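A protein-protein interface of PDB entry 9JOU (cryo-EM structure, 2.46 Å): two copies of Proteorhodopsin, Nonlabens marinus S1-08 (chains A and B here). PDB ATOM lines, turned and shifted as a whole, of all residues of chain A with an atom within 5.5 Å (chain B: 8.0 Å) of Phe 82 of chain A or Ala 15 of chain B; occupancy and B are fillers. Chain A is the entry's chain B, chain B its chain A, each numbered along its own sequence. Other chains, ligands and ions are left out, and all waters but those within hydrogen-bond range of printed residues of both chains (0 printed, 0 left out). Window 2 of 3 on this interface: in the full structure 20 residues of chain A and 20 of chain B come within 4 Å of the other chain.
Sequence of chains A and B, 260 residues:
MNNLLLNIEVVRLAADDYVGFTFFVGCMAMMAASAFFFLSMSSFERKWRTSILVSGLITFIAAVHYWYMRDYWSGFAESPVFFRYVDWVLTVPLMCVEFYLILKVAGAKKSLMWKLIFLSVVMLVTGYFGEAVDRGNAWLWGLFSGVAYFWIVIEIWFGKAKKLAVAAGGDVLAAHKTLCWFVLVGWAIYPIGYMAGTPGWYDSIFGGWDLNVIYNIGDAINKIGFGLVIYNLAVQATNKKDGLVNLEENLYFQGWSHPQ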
ATOM      1  N   PRO A  80      17.078   1.552  18.647  1.00  0.00           N
ATOM      2  CA  PRO A  80      15.681   1.246  18.945  1.00  0.00           C
ATOM      3  C   PRO A  80      14.733   1.699  17.840  1.00  0.00           C
ATOM      4  O   PRO A  80      14.880   2.793  17.298  1.00  0.00           O
ATOM      5  CB  PRO A  80      15.420   1.985  20.244  1.00  0.00           C
ATOM      6  CG  PRO A  80      16.449   3.106  20.230  1.00  0.00           C
ATOM      7  CD  PRO A  80      17.661   2.512  19.602  1.00  0.00           C
ATOM      8  N   VAL A  81      13.770   0.839  17.509  1.00  0.00           N
ATOM      9  CA  VAL A  81      12.986   0.994  16.296  1.00  0.00           C
ATOM     10  C   VAL A  81      12.108   2.234  16.413  1.00  0.00           C
ATOM     11  O   VAL A  81      11.925   2.939  15.426  1.00  0.00           O
ATOM     12  CB  VAL A  81      12.132  -0.237  15.961  1.00  0.00           C
ATOM     13  CG1 VAL A  81      11.181  -0.600  17.099  1.00  0.00           C
ATOM     14  CG2 VAL A  81      11.382  -0.035  14.649  1.00  0.00           C
ATOM     15  N   PHE A  82      11.573   2.475  17.611  1.00  0.00           N
ATOM     16  CA  PHE A  82      10.671   3.590  17.846  1.00  0.00           C
ATOM     17  C   PHE A  82      11.345   4.913  17.485  1.00  0.00           C
ATOM     18  O   PHE A  82      10.681   5.831  17.007  1.00  0.00           O
ATOM     19  CB  PHE A  82      10.172   3.634  19.287  1.00  0.00           C
ATOM     20  CG  PHE A  82      11.195   4.203  20.250  1.00  0.00           C
ATOM     21  CD1 PHE A  82      11.324   5.574  20.435  1.00  0.00           C
ATOM     22  CD2 PHE A  82      12.010   3.352  20.981  1.00  0.00           C
ATOM     23  CE1 PHE A  82      12.262   6.077  21.322  1.00  0.00           C
ATOM     24  CE2 PHE A  82      12.919   3.858  21.892  1.00  0.00           C
ATOM     25  CZ  PHE A  82      13.062   5.216  22.044  1.00  0.00           C
ATOM     26  N   PHE A  83      12.668   4.988  17.677  1.00  0.00           N
ATOM     27  CA  PHE A  83      13.421   6.202  17.402  1.00  0.00           C
ATOM     28  C   PHE A  83      13.350   6.552  15.913  1.00  0.00           C
ATOM     29  O   PHE A  83      13.356   7.719  15.537  1.00  0.00           O
ATOM     30  CB  PHE A  83      14.864   6.022  17.870  1.00  0.00           C
ATOM     31  CG  PHE A  83      15.633   7.321  18.049  1.00  0.00           C
ATOM     32  CD1 PHE A  83      15.135   8.341  18.853  1.00  0.00           C
ATOM     33  CD2 PHE A  83      16.840   7.532  17.388  1.00  0.00           C
ATOM     34  CE1 PHE A  83      15.848   9.513  19.031  1.00  0.00           C
ATOM     35  CE2 PHE A  83      17.556   8.699  17.581  1.00  0.00           C
ATOM     36  CZ  PHE A  83      17.045   9.695  18.378  1.00  0.00           C
ATOM     37  N   ARG A  84      13.275   5.546  15.047  1.00  0.00           N
ATOM     38  CA  ARG A  84      13.142   5.815  13.628  1.00  0.00           C
ATOM     39  C   ARG A  84      11.889   6.636  13.368  1.00  0.00           C
ATOM     40  O   ARG A  84      11.829   7.353  12.373  1.00  0.00           O
ATOM     41  CB  ARG A  84      13.136   4.514  12.816  1.00  0.00           C
ATOM     42  CG  ARG A  84      14.420   3.713  12.929  1.00  0.00           C
ATOM     43  CD  ARG A  84      14.563   2.636  11.877  1.00  0.00           C
ATOM     44  NE  ARG A  84      15.850   1.940  12.015  1.00  0.00           N
ATOM     45  CZ  ARG A  84      16.906   2.109  11.220  1.00  0.00           C
ATOM     46  NH1 ARG A  84      16.880   2.975  10.222  1.00  0.00           N
ATOM     47  NH2 ARG A  84      18.003   1.417  11.436  1.00  0.00           N
ATOM     48  N   TYR A  85      10.874   6.512  14.243  1.00  0.00           N
ATOM     49  CA  TYR A  85       9.576   7.112  13.987  1.00  0.00           C
ATOM     50  C   TYR A  85       9.714   8.626  13.924  1.00  0.00           C
ATOM     51  O   TYR A  85       9.026   9.267  13.126  1.00  0.00           O
ATOM     52  CB  TYR A  85       8.528   6.678  14.998  1.00  0.00           C
ATOM     53  CG  TYR A  85       7.905   5.318  14.707  1.00  0.00           C
ATOM     54  CD1 TYR A  85       6.795   5.181  13.885  1.00  0.00           C
ATOM     55  CD2 TYR A  85       8.419   4.166  15.278  1.00  0.00           C
ATOM     56  CE1 TYR A  85       6.212   3.941  13.657  1.00  0.00           C
ATOM     57  CE2 TYR A  85       7.850   2.920  15.054  1.00  0.00           C
ATOM     58  CZ  TYR A  85       6.742   2.807  14.240  1.00  0.00           C
ATOM     59  OH  TYR A  85       6.198   1.586  13.985  1.00  0.00           O
ATOM     60  N   VAL A  86      10.651   9.163  14.724  1.00  0.00           N
ATOM     61  CA  VAL A  86      11.051  10.568  14.681  1.00  0.00           C
ATOM     62  C   VAL A  86      11.155  11.045  13.238  1.00  0.00           C
ATOM     63  O   VAL A  86      10.685  12.129  12.899  1.00  0.00           O
ATOM     64  CB  VAL A  86      12.393  10.821  15.385  1.00  0.00           C
ATOM     65  CG1 VAL A  86      12.880  12.227  15.113  1.00  0.00           C
ATOM     66  CG2 VAL A  86      12.338  10.566  16.890  1.00  0.00           C
ATOM     67  N   TYR A 128       3.324   4.256  16.131  1.00  0.00           N
ATOM     68  CA  TYR A 128       4.077   4.690  17.301  1.00  0.00           C
ATOM     69  C   TYR A 128       3.409   4.230  18.592  1.00  0.00           C
ATOM     70  O   TYR A 128       4.104   3.877  19.537  1.00  0.00           O
ATOM     71  CB  TYR A 128       4.254   6.212  17.297  1.00  0.00           C
ATOM     72  CG  TYR A 128       5.013   6.721  18.516  1.00  0.00           C
ATOM     73  CD1 TYR A 128       6.350   6.394  18.715  1.00  0.00           C
ATOM     74  CD2 TYR A 128       4.396   7.522  19.467  1.00  0.00           C
ATOM     75  CE1 TYR A 128       7.047   6.834  19.830  1.00  0.00           C
ATOM     76  CE2 TYR A 128       5.094   8.002  20.568  1.00  0.00           C
ATOM     77  CZ  TYR A 128       6.423   7.652  20.750  1.00  0.00           C
ATOM     78  OH  TYR A 128       7.142   8.052  21.836  1.00  0.00           O
ATOM     79  N   GLU A 131       4.038   0.570  19.099  1.00  0.00           N
ATOM     80  CA  GLU A 131       5.427   0.211  19.346  1.00  0.00           C
ATOM     81  C   GLU A 131       5.999   0.836  20.619  1.00  0.00           C
ATOM     82  O   GLU A 131       7.044   0.401  21.097  1.00  0.00           O
ATOM     83  CB  GLU A 131       6.277   0.592  18.132  1.00  0.00           C
ATOM     84  CG  GLU A 131       5.844  -0.117  16.852  1.00  0.00           C
ATOM     85  CD  GLU A 131       6.955  -0.599  15.924  1.00  0.00           C
ATOM     86  OE1 GLU A 131       7.871  -1.204  16.514  1.00  0.00           O
ATOM     87  OE2 GLU A 131       6.923  -0.460  14.677  1.00  0.00           O
ATOM     88  N   ALA A 132       5.345   1.866  21.178  1.00  0.00           N
ATOM     89  CA  ALA A 132       5.906   2.639  22.276  1.00  0.00           C
ATOM     90  C   ALA A 132       5.087   2.511  23.563  1.00  0.00           C
ATOM     91  O   ALA A 132       5.637   2.127  24.591  1.00  0.00           O
ATOM     92  CB  ALA A 132       6.022   4.079  21.840  1.00  0.00           C
ATOM     93  N   ARG B  12      21.047   7.420  27.186  1.00  0.00           N
ATOM     94  CA  ARG B  12      20.219   6.486  26.438  1.00  0.00           C
ATOM     95  C   ARG B  12      18.754   6.866  26.637  1.00  0.00           C
ATOM     96  O   ARG B  12      18.344   7.208  27.743  1.00  0.00           O
ATOM     97  CB  ARG B  12      20.504   5.042  26.880  1.00  0.00           C
ATOM     98  CG  ARG B  12      19.463   3.994  26.513  1.00  0.00           C
ATOM     99  CD  ARG B  12      19.559   2.725  27.328  1.00  0.00           C
ATOM    100  NE  ARG B  12      20.528   1.820  26.703  1.00  0.00           N
ATOM    101  CZ  ARG B  12      21.818   1.701  27.005  1.00  0.00           C
ATOM    102  NH1 ARG B  12      22.396   2.536  27.852  1.00  0.00           N
ATOM    103  NH2 ARG B  12      22.543   0.757  26.426  1.00  0.00           N
ATOM    104  N   LEU B  13      17.972   6.800  25.552  1.00  0.00           N
ATOM    105  CA  LEU B  13      16.568   7.176  25.596  1.00  0.00           C
ATOM    106  C   LEU B  13      15.743   5.917  25.833  1.00  0.00           C
ATOM    107  O   LEU B  13      16.169   4.814  25.527  1.00  0.00           O
ATOM    108  CB  LEU B  13      16.114   7.947  24.353  1.00  0.00           C
ATOM    109  CG  LEU B  13      15.941   7.168  23.051  1.00  0.00           C
ATOM    110  CD1 LEU B  13      15.281   8.095  22.046  1.00  0.00           C
ATOM    111  CD2 LEU B  13      17.240   6.619  22.504  1.00  0.00           C
ATOM    112  N   ALA B  14      14.505   6.117  26.304  1.00  0.00           N
ATOM    113  CA  ALA B  14      13.546   5.056  26.544  1.00  0.00           C
ATOM    114  C   ALA B  14      12.320   5.249  25.652  1.00  0.00           C
ATOM    115  O   ALA B  14      12.087   6.343  25.153  1.00  0.00           O
ATOM    116  CB  ALA B  14      13.182   5.080  28.006  1.00  0.00           C
ATOM    117  N   ALA B  15      11.560   4.170  25.440  1.00  0.00           N
ATOM    118  CA  ALA B  15      10.429   4.171  24.527  1.00  0.00           C
ATOM    119  C   ALA B  15       9.290   5.042  25.058  1.00  0.00           C
ATOM    120  O   ALA B  15       8.574   5.666  24.274  1.00  0.00           O
ATOM    121  CB  ALA B  15       9.970   2.749  24.295  1.00  0.00           C
ATOM    122  N   ASP B  16       9.140   5.092  26.394  1.00  0.00           N
ATOM    123  CA  ASP B  16       8.006   5.754  27.028  1.00  0.00           C
ATOM    124  C   ASP B  16       8.298   7.232  27.285  1.00  0.00           C
ATOM    125  O   ASP B  16       7.457   7.938  27.834  1.00  0.00           O
ATOM    126  CB  ASP B  16       7.577   5.019  28.289  1.00  0.00           C
ATOM    127  CG  ASP B  16       8.498   5.081  29.500  1.00  0.00           C
ATOM    128  OD1 ASP B  16       9.622   5.624  29.377  1.00  0.00           O
ATOM    129  OD2 ASP B  16       8.055   4.631  30.566  1.00  0.00           O
ATOM    130  N   ASP B  17       9.506   7.695  26.936  1.00  0.00           N
ATOM    131  CA  ASP B  17       9.885   9.092  27.096  1.00  0.00           C
ATOM    132  C   ASP B  17       9.240   9.907  25.969  1.00  0.00           C
ATOM    133  O   ASP B  17       9.847  10.184  24.926  1.00  0.00           O
ATOM    134  CB  ASP B  17      11.397   9.227  27.185  1.00  0.00           C
ATOM    135  CG  ASP B  17      11.944  10.621  27.453  1.00  0.00           C
ATOM    136  OD1 ASP B  17      11.131  11.518  27.708  1.00  0.00           O
ATOM    137  OD2 ASP B  17      13.184  10.796  27.409  1.00  0.00           O
ATOM    138  N   TYR B  18       7.997  10.318  26.217  1.00  0.00           N
ATOM    139  CA  TYR B  18       7.204  11.031  25.234  1.00  0.00           C
ATOM    140  C   TYR B  18       7.678  12.469  25.105  1.00  0.00           C
ATOM    141  O   TYR B  18       7.442  13.102  24.079  1.00  0.00           O
ATOM    142  CB  TYR B  18       5.735  11.088  25.661  1.00  0.00           C
ATOM    143  CG  TYR B  18       5.183   9.774  26.179  1.00  0.00           C
ATOM    144  CD1 TYR B  18       5.459   8.578  25.528  1.00  0.00           C
ATOM    145  CD2 TYR B  18       4.425   9.728  27.341  1.00  0.00           C
ATOM    146  CE1 TYR B  18       4.968   7.372  26.002  1.00  0.00           C
ATOM    147  CE2 TYR B  18       3.929   8.528  27.826  1.00  0.00           C
ATOM    148  CZ  TYR B  18       4.207   7.347  27.158  1.00  0.00           C
ATOM    149  OH  TYR B  18       3.699   6.175  27.640  1.00  0.00           O
ATOM    150  N   VAL B  19       8.265  12.999  26.182  1.00  0.00           N
ATOM    151  CA  VAL B  19       8.839  14.330  26.129  1.00  0.00           C
ATOM    152  C   VAL B  19      10.012  14.277  25.158  1.00  0.00           C
ATOM    153  O   VAL B  19      10.068  15.068  24.217  1.00  0.00           O
ATOM    154  CB  VAL B  19       9.265  14.837  27.521  1.00  0.00           C
ATOM    155  CG1 VAL B  19       9.878  16.227  27.450  1.00  0.00           C
ATOM    156  CG2 VAL B  19       8.105  14.797  28.514  1.00  0.00           C
ATOM    157  N   GLY B  20      10.916  13.308  25.369  1.00  0.00           N
ATOM    158  CA  GLY B  20      12.049  13.123  24.480  1.00  0.00           C
ATOM    159  C   GLY B  20      11.593  13.189  23.028  1.00  0.00           C
ATOM    160  O   GLY B  20      12.049  14.013  22.229  1.00  0.00           O
ATOM    161  N   PHE B  21      10.611  12.356  22.728  1.00  0.00           N
ATOM    162  CA  PHE B  21      10.184  12.179  21.359  1.00  0.00           C
ATOM    163  C   PHE B  21       9.735  13.525  20.784  1.00  0.00           C
ATOM    164  O   PHE B  21       9.978  13.848  19.622  1.00  0.00           O
ATOM    165  CB  PHE B  21       9.136  11.056  21.357  1.00  0.00           C
ATOM    166  CG  PHE B  21       8.792  10.662  19.926  1.00  0.00           C
ATOM    167  CD1 PHE B  21       9.556   9.730  19.225  1.00  0.00           C
ATOM    168  CD2 PHE B  21       7.746  11.287  19.261  1.00  0.00           C
ATOM    169  CE1 PHE B  21       9.273   9.438  17.899  1.00  0.00           C
ATOM    170  CE2 PHE B  21       7.452  10.972  17.945  1.00  0.00           C
ATOM    171  CZ  PHE B  21       8.225  10.060  17.261  1.00  0.00           C
ATOM    172  N   PHE B  24      12.574  15.862  19.840  1.00  0.00           N
ATOM    173  CA  PHE B  24      13.237  15.466  18.604  1.00  0.00           C
ATOM    174  C   PHE B  24      12.366  15.762  17.387  1.00  0.00           C
ATOM    175  O   PHE B  24      12.856  16.151  16.340  1.00  0.00           O
ATOM    176  CB  PHE B  24      13.572  13.983  18.623  1.00  0.00           C
ATOM    177  CG  PHE B  24      14.925  13.678  19.234  1.00  0.00           C
ATOM    178  CD1 PHE B  24      15.055  13.505  20.600  1.00  0.00           C
ATOM    179  CD2 PHE B  24      16.061  13.561  18.431  1.00  0.00           C
ATOM    180  CE1 PHE B  24      16.285  13.201  21.157  1.00  0.00           C
ATOM    181  CE2 PHE B  24      17.287  13.263  18.993  1.00  0.00           C
ATOM    182  CZ  PHE B  24      17.397  13.085  20.355  1.00  0.00           C
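Phe 82 of chain A touches Leu 13 of chain B. CZ of Phe 82 of chain A touches O of Ala 14 of chain B (3.4 Å). Ala 15 of chain B touches Phe 82 of chain A (CA to CE2, 3.6 Å). Phe 82 of chain A touches Phe 21 of chain B (O to CE1, 3.97 Å). Phe 83 of chain A touches Leu 13 of chain B (CD1 to CD1, 3.2 Å). CZ of Phe 83 of chain A touches CE2 of Phe 24 of chain B, at 3.6 Å. Tyr 85 of chain A touches Phe 21 of chain B. Val 86 of chain A touches Phe 21 of chain B (CG2 to CE1, 3.4 Å). Tyr 128 of chain A touches Ala 15 of chain B. Ala 132 of chain A touches Ala 15 of chain B (CB to O, 3.9 Å).
No residue of chain B comes within 4 Å of Val 81 of chain A. Of the printed residues of chain B, Phe 82 of chain A touches Leu 13 (3.6 Å), Ala 14 (3.4 Å), Ala 15 (3.6 Å) and Phe 21 (3.97 Å). Printed residues of chain B within 4 Å of Phe 83 of chain A: Leu 13 (3.2 Å) and Phe 24 (3.6 Å). Printed residues of chain B within 4 Å of Tyr 85 of chain A: Phe 21 (3.9 Å). Glu 131 of chain A touches none of the printed residues of chain B. Of the printed residues of chain A, Leu 13 of chain B touches Phe 82 (3.6 Å) and Phe 83 (3.2 Å). Of the printed residues of chain A, Ala 14 of chain B touches Phe 82. Val 19 of chain B touches none of the printed residues of chain A. The nearest residue of chain B that does not touch Phe 82 of chain A is Asp 16 of chain B (5.9 Å).
Of the 11 printed residues of chain B, 5 touch a printed residue of chain A. Hydrophobic or aromatic side chains of chain A within 4 Å of the printed part of chain B: Phe 82, Phe 83, Val 86, Tyr 128 and Ala 132. Among the printed residues, 12 pairs touch across the chains.
No position is printed for both chains. Of the 12 pairs that touch across the chains among the printed residues, none has its exchanged pair printed and touching as well.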
